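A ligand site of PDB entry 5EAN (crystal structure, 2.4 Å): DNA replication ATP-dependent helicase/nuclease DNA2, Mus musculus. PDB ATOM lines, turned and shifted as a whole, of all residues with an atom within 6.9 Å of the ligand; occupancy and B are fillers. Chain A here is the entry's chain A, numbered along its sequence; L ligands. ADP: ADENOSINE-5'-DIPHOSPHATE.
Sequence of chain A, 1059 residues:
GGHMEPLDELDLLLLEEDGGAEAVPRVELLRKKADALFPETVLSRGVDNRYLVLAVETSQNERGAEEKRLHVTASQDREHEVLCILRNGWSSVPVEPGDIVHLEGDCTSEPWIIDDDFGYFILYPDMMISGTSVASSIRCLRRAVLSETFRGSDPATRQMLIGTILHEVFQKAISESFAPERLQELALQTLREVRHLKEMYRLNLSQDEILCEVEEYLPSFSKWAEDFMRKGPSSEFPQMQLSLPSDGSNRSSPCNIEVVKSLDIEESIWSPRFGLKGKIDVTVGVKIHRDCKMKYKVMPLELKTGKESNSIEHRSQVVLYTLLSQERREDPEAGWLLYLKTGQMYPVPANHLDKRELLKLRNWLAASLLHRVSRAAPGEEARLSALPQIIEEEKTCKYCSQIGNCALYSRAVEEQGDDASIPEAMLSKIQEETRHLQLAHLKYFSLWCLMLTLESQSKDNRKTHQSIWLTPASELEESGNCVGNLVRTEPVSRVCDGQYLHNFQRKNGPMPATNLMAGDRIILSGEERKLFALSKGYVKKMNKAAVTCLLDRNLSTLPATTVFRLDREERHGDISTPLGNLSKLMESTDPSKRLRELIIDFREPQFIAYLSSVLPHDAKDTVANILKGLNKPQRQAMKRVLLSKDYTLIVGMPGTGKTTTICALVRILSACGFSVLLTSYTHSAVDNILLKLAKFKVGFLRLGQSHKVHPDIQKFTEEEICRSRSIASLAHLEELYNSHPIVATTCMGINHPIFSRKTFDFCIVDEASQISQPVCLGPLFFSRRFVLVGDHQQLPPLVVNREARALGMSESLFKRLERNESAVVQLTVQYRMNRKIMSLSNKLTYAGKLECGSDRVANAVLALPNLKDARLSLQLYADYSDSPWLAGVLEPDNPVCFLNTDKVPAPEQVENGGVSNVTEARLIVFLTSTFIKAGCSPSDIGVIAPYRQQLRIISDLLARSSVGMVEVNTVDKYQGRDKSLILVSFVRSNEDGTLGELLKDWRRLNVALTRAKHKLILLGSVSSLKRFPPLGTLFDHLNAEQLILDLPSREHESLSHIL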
ATOM      1  N   LYS A 628       4.547   0.930  13.928  1.00  0.00           N
ATOM      2  CA  LYS A 628       3.770  -0.168  13.313  1.00  0.00           C
ATOM      3  C   LYS A 628       3.251  -1.113  14.376  1.00  0.00           C
ATOM      4  O   LYS A 628       2.116  -1.541  14.284  1.00  0.00           O
ATOM      5  CB  LYS A 628       4.575  -0.966  12.291  1.00  0.00           C
ATOM      6  CG  LYS A 628       4.686  -0.345  10.906  1.00  0.00           C
ATOM      7  CD  LYS A 628       5.842  -0.993  10.165  1.00  0.00           C
ATOM      8  CE  LYS A 628       6.066  -0.392   8.785  1.00  0.00           C
ATOM      9  NZ  LYS A 628       7.517  -0.076   8.544  1.00  0.00           N
ATOM     10  N   GLY A 629       4.067  -1.418  15.385  1.00  0.00           N
ATOM     11  CA  GLY A 629       3.607  -2.213  16.523  1.00  0.00           C
ATOM     12  C   GLY A 629       2.433  -1.656  17.354  1.00  0.00           C
ATOM     13  O   GLY A 629       1.786  -2.391  18.090  1.00  0.00           O
ATOM     14  N   LEU A 630       2.150  -0.369  17.235  1.00  0.00           N
ATOM     15  CA  LEU A 630       1.172   0.252  18.102  1.00  0.00           C
ATOM     16  C   LEU A 630      -0.218   0.267  17.489  1.00  0.00           C
ATOM     17  O   LEU A 630      -0.366   0.224  16.257  1.00  0.00           O
ATOM     18  CB  LEU A 630       1.628   1.683  18.456  1.00  0.00           C
ATOM     19  CG  LEU A 630       3.037   1.820  19.048  1.00  0.00           C
ATOM     20  CD1 LEU A 630       3.387   3.297  19.277  1.00  0.00           C
ATOM     21  CD2 LEU A 630       3.203   1.015  20.327  1.00  0.00           C
ATOM     22  N   ASN A 631      -1.238   0.335  18.348  1.00  0.00           N
ATOM     23  CA  ASN A 631      -2.602   0.575  17.858  1.00  0.00           C
ATOM     24  C   ASN A 631      -2.766   2.082  17.546  1.00  0.00           C
ATOM     25  O   ASN A 631      -1.866   2.897  17.848  1.00  0.00           O
ATOM     26  CB  ASN A 631      -3.649   0.020  18.837  1.00  0.00           C
ATOM     27  CG  ASN A 631      -3.592   0.677  20.240  1.00  0.00           C
ATOM     28  OD1 ASN A 631      -3.604   1.918  20.380  1.00  0.00           O
ATOM     29  ND2 ASN A 631      -3.552  -0.164  21.267  1.00  0.00           N
ATOM     30  N   LYS A 632      -3.875   2.454  16.911  1.00  0.00           N
ATOM     31  CA  LYS A 632      -4.111   3.830  16.441  1.00  0.00           C
ATOM     32  C   LYS A 632      -4.074   4.900  17.559  1.00  0.00           C
ATOM     33  O   LYS A 632      -3.346   5.900  17.416  1.00  0.00           O
ATOM     34  CB  LYS A 632      -5.426   3.911  15.629  1.00  0.00           C
ATOM     35  CG  LYS A 632      -5.268   4.169  14.136  1.00  0.00           C
ATOM     36  CD  LYS A 632      -4.806   2.953  13.328  1.00  0.00           C
ATOM     37  CE  LYS A 632      -4.478   3.321  11.884  1.00  0.00           C
ATOM     38  NZ  LYS A 632      -5.669   3.564  11.001  1.00  0.00           N
ATOM     39  N   GLN A 634      -2.575   4.732  20.364  1.00  0.00           N
ATOM     40  CA  GLN A 634      -1.196   4.756  20.791  1.00  0.00           C
ATOM     41  C   GLN A 634      -0.295   5.583  19.872  1.00  0.00           C
ATOM     42  O   GLN A 634       0.533   6.362  20.354  1.00  0.00           O
ATOM     43  CB  GLN A 634      -0.642   3.351  20.909  1.00  0.00           C
ATOM     44  CG  GLN A 634      -0.975   2.682  22.237  1.00  0.00           C
ATOM     45  CD  GLN A 634      -0.565   1.233  22.228  1.00  0.00           C
ATOM     46  OE1 GLN A 634      -0.455   0.637  21.162  1.00  0.00           O
ATOM     47  NE2 GLN A 634      -0.341   0.663  23.396  1.00  0.00           N
ATOM     48  N   GLY A 655      -5.992  -1.153  31.445  1.00  0.00           N
ATOM     49  CA  GLY A 655      -5.703  -2.260  30.525  1.00  0.00           C
ATOM     50  C   GLY A 655      -5.201  -1.793  29.160  1.00  0.00           C
ATOM     51  O   GLY A 655      -5.022  -2.612  28.270  1.00  0.00           O
ATOM     52  N   THR A 656      -4.993  -0.484  29.001  1.00  0.00           N
ATOM     53  CA  THR A 656      -4.553   0.052  27.717  1.00  0.00           C
ATOM     54  C   THR A 656      -3.026  -0.008  27.467  1.00  0.00           C
ATOM     55  O   THR A 656      -2.549   0.415  26.398  1.00  0.00           O
ATOM     56  CB  THR A 656      -5.060   1.488  27.479  1.00  0.00           C
ATOM     57  OG1 THR A 656      -4.636   2.330  28.552  1.00  0.00           O
ATOM     58  CG2 THR A 656      -6.576   1.511  27.329  1.00  0.00           C
ATOM     59  N   GLY A 657      -2.269  -0.554  28.407  1.00  0.00           N
ATOM     60  CA  GLY A 657      -0.864  -0.811  28.182  1.00  0.00           C
ATOM     61  C   GLY A 657      -0.025   0.447  28.324  1.00  0.00           C
ATOM     62  O   GLY A 657       0.688   0.858  27.390  1.00  0.00           O
ATOM     63  N   LYS A 658      -0.151   1.039  29.506  1.00  0.00           N
ATOM     64  CA  LYS A 658       0.544   2.223  29.930  1.00  0.00           C
ATOM     65  C   LYS A 658       2.040   2.015  29.744  1.00  0.00           C
ATOM     66  O   LYS A 658       2.707   2.846  29.130  1.00  0.00           O
ATOM     67  CB  LYS A 658       0.237   2.424  31.418  1.00  0.00           C
ATOM     68  CG  LYS A 658       0.222   3.841  31.907  1.00  0.00           C
ATOM     69  CD  LYS A 658      -0.817   3.947  33.021  1.00  0.00           C
ATOM     70  CE  LYS A 658      -0.271   3.817  34.465  1.00  0.00           C
ATOM     71  NZ  LYS A 658       0.879   2.874  34.694  1.00  0.00           N
ATOM     72  N   THR A 659       2.555   0.894  30.259  1.00  0.00           N
ATOM     73  CA  THR A 659       3.984   0.706  30.277  1.00  0.00           C
ATOM     74  C   THR A 659       4.510   0.434  28.873  1.00  0.00           C
ATOM     75  O   THR A 659       5.558   0.960  28.523  1.00  0.00           O
ATOM     76  CB  THR A 659       4.470  -0.282  31.350  1.00  0.00           C
ATOM     77  OG1 THR A 659       4.094  -1.591  30.987  1.00  0.00           O
ATOM     78  CG2 THR A 659       3.836   0.050  32.679  1.00  0.00           C
ATOM     79  N   THR A 660       3.743  -0.298  28.071  1.00  0.00           N
ATOM     80  CA  THR A 660       4.044  -0.516  26.652  1.00  0.00           C
ATOM     81  C   THR A 660       4.121   0.806  25.896  1.00  0.00           C
ATOM     82  O   THR A 660       4.996   0.985  25.053  1.00  0.00           O
ATOM     83  CB  THR A 660       2.984  -1.460  25.997  1.00  0.00           C
ATOM     84  OG1 THR A 660       2.973  -2.694  26.716  1.00  0.00           O
ATOM     85  CG2 THR A 660       3.294  -1.774  24.551  1.00  0.00           C
ATOM     86  N   THR A 661       3.217   1.716  26.215  1.00  0.00           N
ATOM     87  CA  THR A 661       3.076   2.969  25.482  1.00  0.00           C
ATOM     88  C   THR A 661       4.216   3.935  25.832  1.00  0.00           C
ATOM     89  O   THR A 661       4.722   4.621  24.957  1.00  0.00           O
ATOM     90  CB  THR A 661       1.682   3.593  25.741  1.00  0.00           C
ATOM     91  OG1 THR A 661       0.675   2.662  25.346  1.00  0.00           O
ATOM     92  CG2 THR A 661       1.468   4.900  24.960  1.00  0.00           C
ATOM     93  N   ASN A 688       8.999  -0.714  35.977  1.00  0.00           N
ATOM     94  CA  ASN A 688       8.230  -1.513  35.013  1.00  0.00           C
ATOM     95  C   ASN A 688       8.515  -1.109  33.575  1.00  0.00           C
ATOM     96  O   ASN A 688       8.662  -1.981  32.701  1.00  0.00           O
ATOM     97  CB  ASN A 688       6.715  -1.467  35.304  1.00  0.00           C
ATOM     98  CG  ASN A 688       6.306  -2.419  36.420  1.00  0.00           C
ATOM     99  OD1 ASN A 688       7.094  -3.255  36.870  1.00  0.00           O
ATOM    100  ND2 ASN A 688       5.065  -2.292  36.892  1.00  0.00           N
ATOM    101  N   LYS A 692      10.952  -3.202  30.273  1.00  0.00           N
ATOM    102  CA  LYS A 692      10.680  -3.251  28.824  1.00  0.00           C
ATOM    103  C   LYS A 692      11.793  -2.651  27.999  1.00  0.00           C
ATOM    104  O   LYS A 692      12.251  -3.252  27.028  1.00  0.00           O
ATOM    105  CB  LYS A 692       9.346  -2.614  28.461  1.00  0.00           C
ATOM    106  CG  LYS A 692       8.160  -3.321  29.038  1.00  0.00           C
ATOM    107  CD  LYS A 692       6.889  -2.851  28.376  1.00  0.00           C
ATOM    108  CE  LYS A 692       5.730  -3.674  28.899  1.00  0.00           C
ATOM    109  NZ  LYS A 692       5.519  -4.889  28.069  1.00  0.00           N
ATOM    110  N   VAL A 829      -7.818   1.318  23.456  1.00  0.00           N
ATOM    111  CA  VAL A 829      -7.764  -0.105  23.160  1.00  0.00           C
ATOM    112  C   VAL A 829      -7.176  -0.833  24.375  1.00  0.00           C
ATOM    113  O   VAL A 829      -6.005  -0.593  24.738  1.00  0.00           O
ATOM    114  CB  VAL A 829      -6.950  -0.415  21.890  1.00  0.00           C
ATOM    115  CG1 VAL A 829      -6.949  -1.905  21.610  1.00  0.00           C
ATOM    116  CG2 VAL A 829      -7.491   0.345  20.689  1.00  0.00           C
ATOM    117  N   GLN A 830      -7.971  -1.699  25.013  1.00  0.00           N
ATOM    118  CA  GLN A 830      -7.530  -2.406  26.238  1.00  0.00           C
ATOM    119  C   GLN A 830      -7.373  -3.922  26.046  1.00  0.00           C
ATOM    120  O   GLN A 830      -8.158  -4.550  25.305  1.00  0.00           O
ATOM    121  CB  GLN A 830      -8.386  -2.073  27.464  1.00  0.00           C
ATOM    122  CG  GLN A 830      -9.841  -2.577  27.437  1.00  0.00           C
ATOM    123  CD  GLN A 830      -9.994  -4.029  27.869  1.00  0.00           C
ATOM    124  OE1 GLN A 830      -9.189  -4.547  28.643  1.00  0.00           O
ATOM    125  NE2 GLN A 830     -11.020  -4.690  27.383  1.00  0.00           N
ATOM    126  N   TYR A 831      -6.396  -4.488  26.749  1.00  0.00           N
ATOM    127  CA  TYR A 831      -6.030  -5.884  26.564  1.00  0.00           C
ATOM    128  C   TYR A 831      -6.200  -6.704  27.831  1.00  0.00           C
ATOM    129  O   TYR A 831      -5.619  -7.775  27.961  1.00  0.00           O
ATOM    130  CB  TYR A 831      -4.579  -5.969  26.023  1.00  0.00           C
ATOM    131  CG  TYR A 831      -4.366  -5.184  24.750  1.00  0.00           C
ATOM    132  CD1 TYR A 831      -4.224  -3.771  24.775  1.00  0.00           C
ATOM    133  CD2 TYR A 831      -4.316  -5.849  23.510  1.00  0.00           C
ATOM    134  CE1 TYR A 831      -4.051  -3.052  23.599  1.00  0.00           C
ATOM    135  CE2 TYR A 831      -4.120  -5.135  22.326  1.00  0.00           C
ATOM    136  CZ  TYR A 831      -3.992  -3.752  22.369  1.00  0.00           C
ATOM    137  OH  TYR A 831      -3.811  -3.036  21.204  1.00  0.00           O
ATOM    138  N   ARG A 832      -7.016  -6.209  28.769  1.00  0.00           N
ATOM    139  CA  ARG A 832      -7.193  -6.881  30.041  1.00  0.00           C
ATOM    140  C   ARG A 832      -8.550  -7.601  30.156  1.00  0.00           C
ATOM    141  O   ARG A 832      -8.583  -8.799  30.388  1.00  0.00           O
ATOM    142  CB  ARG A 832      -7.042  -5.863  31.162  1.00  0.00           C
ATOM    143  CG  ARG A 832      -7.494  -6.338  32.535  1.00  0.00           C
ATOM    144  CD  ARG A 832      -7.444  -5.188  33.535  1.00  0.00           C
ATOM    145  NE  ARG A 832      -6.079  -4.700  33.601  1.00  0.00           N
ATOM    146  CZ  ARG A 832      -5.718  -3.538  34.142  1.00  0.00           C
ATOM    147  NH1 ARG A 832      -6.615  -2.725  34.710  1.00  0.00           N
ATOM    148  NH2 ARG A 832      -4.449  -3.194  34.106  1.00  0.00           N
ATOM    149  N   GLY A 853      -8.905  -5.271  22.578  1.00  0.00           N
ATOM    150  CA  GLY A 853      -7.845  -5.217  21.613  1.00  0.00           C
ATOM    151  C   GLY A 853      -7.866  -6.330  20.613  1.00  0.00           C
ATOM    152  O   GLY A 853      -7.202  -6.233  19.581  1.00  0.00           O
ATOM    153  N   GLY A 976      -3.058  -0.094  38.607  1.00  0.00           N
ATOM    154  CA  GLY A 976      -2.309  -0.507  37.413  1.00  0.00           C
ATOM    155  C   GLY A 976      -2.067  -2.002  37.248  1.00  0.00           C
ATOM    156  O   GLY A 976      -1.423  -2.412  36.287  1.00  0.00           O
ATOM    157  N   ASP A 978      -3.648  -6.249  37.465  1.00  0.00           N
ATOM    158  CA  ASP A 978      -4.807  -7.089  37.229  1.00  0.00           C
ATOM    159  C   ASP A 978      -4.609  -8.517  37.736  1.00  0.00           C
ATOM    160  O   ASP A 978      -3.518  -8.885  38.136  1.00  0.00           O
ATOM    161  CB  ASP A 978      -5.230  -7.049  35.752  1.00  0.00           C
ATOM    162  CG  ASP A 978      -4.083  -7.313  34.772  1.00  0.00           C
ATOM    163  OD1 ASP A 978      -3.346  -8.308  34.923  1.00  0.00           O
ATOM    164  OD2 ASP A 978      -3.940  -6.527  33.805  1.00  0.00           O
ATOM    165  N   LYS A1013      -9.442  -9.761  34.729  1.00  0.00           N
ATOM    166  CA  LYS A1013      -9.314 -10.160  33.330  1.00  0.00           C
ATOM    167  C   LYS A1013     -10.530 -10.981  32.891  1.00  0.00           C
ATOM    168  O   LYS A1013     -11.189 -10.644  31.907  1.00  0.00           O
ATOM    169  CB  LYS A1013      -8.021 -10.949  33.046  1.00  0.00           C
ATOM    170  CG  LYS A1013      -6.716 -10.270  33.434  1.00  0.00           C
ATOM    171  CD  LYS A1013      -5.485 -11.060  32.970  1.00  0.00           C
ATOM    172  CE  LYS A1013      -5.019 -10.600  31.583  1.00  0.00           C
ATOM    173  NZ  LYS A1013      -3.832 -11.318  31.029  1.00  0.00           N
HETATM  174  PB  ADP L   1       2.804  -6.092  30.287  1.00  0.00           P
HETATM  175  O1B ADP L   1       4.039  -5.803  31.126  1.00  0.00           O
HETATM  176  O2B ADP L   1       3.044  -7.068  29.157  1.00  0.00           O
HETATM  177  O3B ADP L   1       1.558  -6.349  31.105  1.00  0.00           O
HETATM  178  PA  ADP L   1       1.480  -3.574  29.873  1.00  0.00           P
HETATM  179  O1A ADP L   1       1.428  -3.377  31.369  1.00  0.00           O
HETATM  180  O2A ADP L   1       1.793  -2.422  28.963  1.00  0.00           O
HETATM  181  O3A ADP L   1       2.562  -4.715  29.484  1.00  0.00           O
HETATM  182  O5' ADP L   1       0.090  -4.243  29.405  1.00  0.00           O
HETATM  183  C5' ADP L   1      -0.264  -4.238  28.038  1.00  0.00           C
HETATM  184  C4' ADP L   1      -0.670  -5.607  27.544  1.00  0.00           C
HETATM  185  O4' ADP L   1      -1.470  -5.394  26.389  1.00  0.00           O
HETATM  186  C3' ADP L   1       0.546  -6.410  27.105  1.00  0.00           C
HETATM  187  O3' ADP L   1       0.546  -7.670  27.783  1.00  0.00           O
HETATM  188  C2' ADP L   1       0.463  -6.568  25.607  1.00  0.00           C
HETATM  189  O2' ADP L   1       0.343  -7.949  25.258  1.00  0.00           O
HETATM  190  C1' ADP L   1      -0.822  -5.840  25.193  1.00  0.00           C
HETATM  191  N9  ADP L   1      -0.612  -4.681  24.286  1.00  0.00           N
HETATM  192  C8  ADP L   1      -0.445  -3.386  24.621  1.00  0.00           C
HETATM  193  N7  ADP L   1      -0.307  -2.578  23.540  1.00  0.00           N
HETATM  194  C5  ADP L   1      -0.391  -3.385  22.456  1.00  0.00           C
HETATM  195  C6  ADP L   1      -0.335  -3.222  20.978  1.00  0.00           C
HETATM  196  N6  ADP L   1      -0.144  -2.004  20.412  1.00  0.00           N
HETATM  197  N1  ADP L   1      -0.468  -4.337  20.196  1.00  0.00           N
HETATM  198  C2  ADP L   1      -0.662  -5.566  20.734  1.00  0.00           C
HETATM  199  N3  ADP L   1      -0.734  -5.783  22.065  1.00  0.00           N
HETATM  200  C4  ADP L   1      -0.601  -4.762  22.951  1.00  0.00           C
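O of Gly 629 is in hydrogen-bond range of N6 of the ligand.
The side-chain hydroxyl (OG1) of Thr 660 sits at hydrogen-bond distance from an oxygen (O2A) of the ligand (2.6 Å).
NZ of Lys 692 lies within salt-bridge range of O2B of the ligand, 3.5 Å away.
The side-chain amide oxygen (OE1) of Gln 634 lies within hydrogen-bond range of a nitrogen (N6) of the ligand, at 2.8 Å.
The backbone NH (N) of Thr 660 lies within hydrogen-bond range of an oxygen (O2A) of the ligand.
OG1 of Thr 659 is in hydrogen-bond range of O2A of the ligand (3.2 Å).
ND2 of Asn 631 is in hydrogen-bond range of OH of Tyr 831 (2.9 Å).
OG1 of Thr 661 sits at hydrogen-bond distance from NE2 of Gln 634 (3.0 Å).
The backbone NH of Tyr 831 sits at hydrogen-bond distance from the backbone carbonyl oxygen of Gly 655 (2.8 Å).
The side-chain amide oxygen (OE1) of Gln 634 lies within hydrogen-bond range of the backbone NH (N) of Asn 631, 2.9 Å away.
The backbone carbonyl oxygen (O) of Gly 657 sits at hydrogen-bond distance from the side-chain hydroxyl (OG1) of Thr 661, 2.7 Å away.
N6 of the ligand sits close to N of Asn 631 (3.3 Å).
Merely in contact with the ligand: Leu 630 (3.5 Å), Gly 657 (3.2 Å) and Tyr 831 (3.2 Å).
Hydrophobic or aromatic side chains within 4 Å of the ligand: Tyr 831.
Within 4 Å of the ligand: Gly 629, Leu 630, Asn 631, Gln 634, Gly 657, Thr 659, Thr 660, Lys 692 and Tyr 831.
The nearest printed residue that does not touch the ligand is Lys 658 (4.01 Å).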
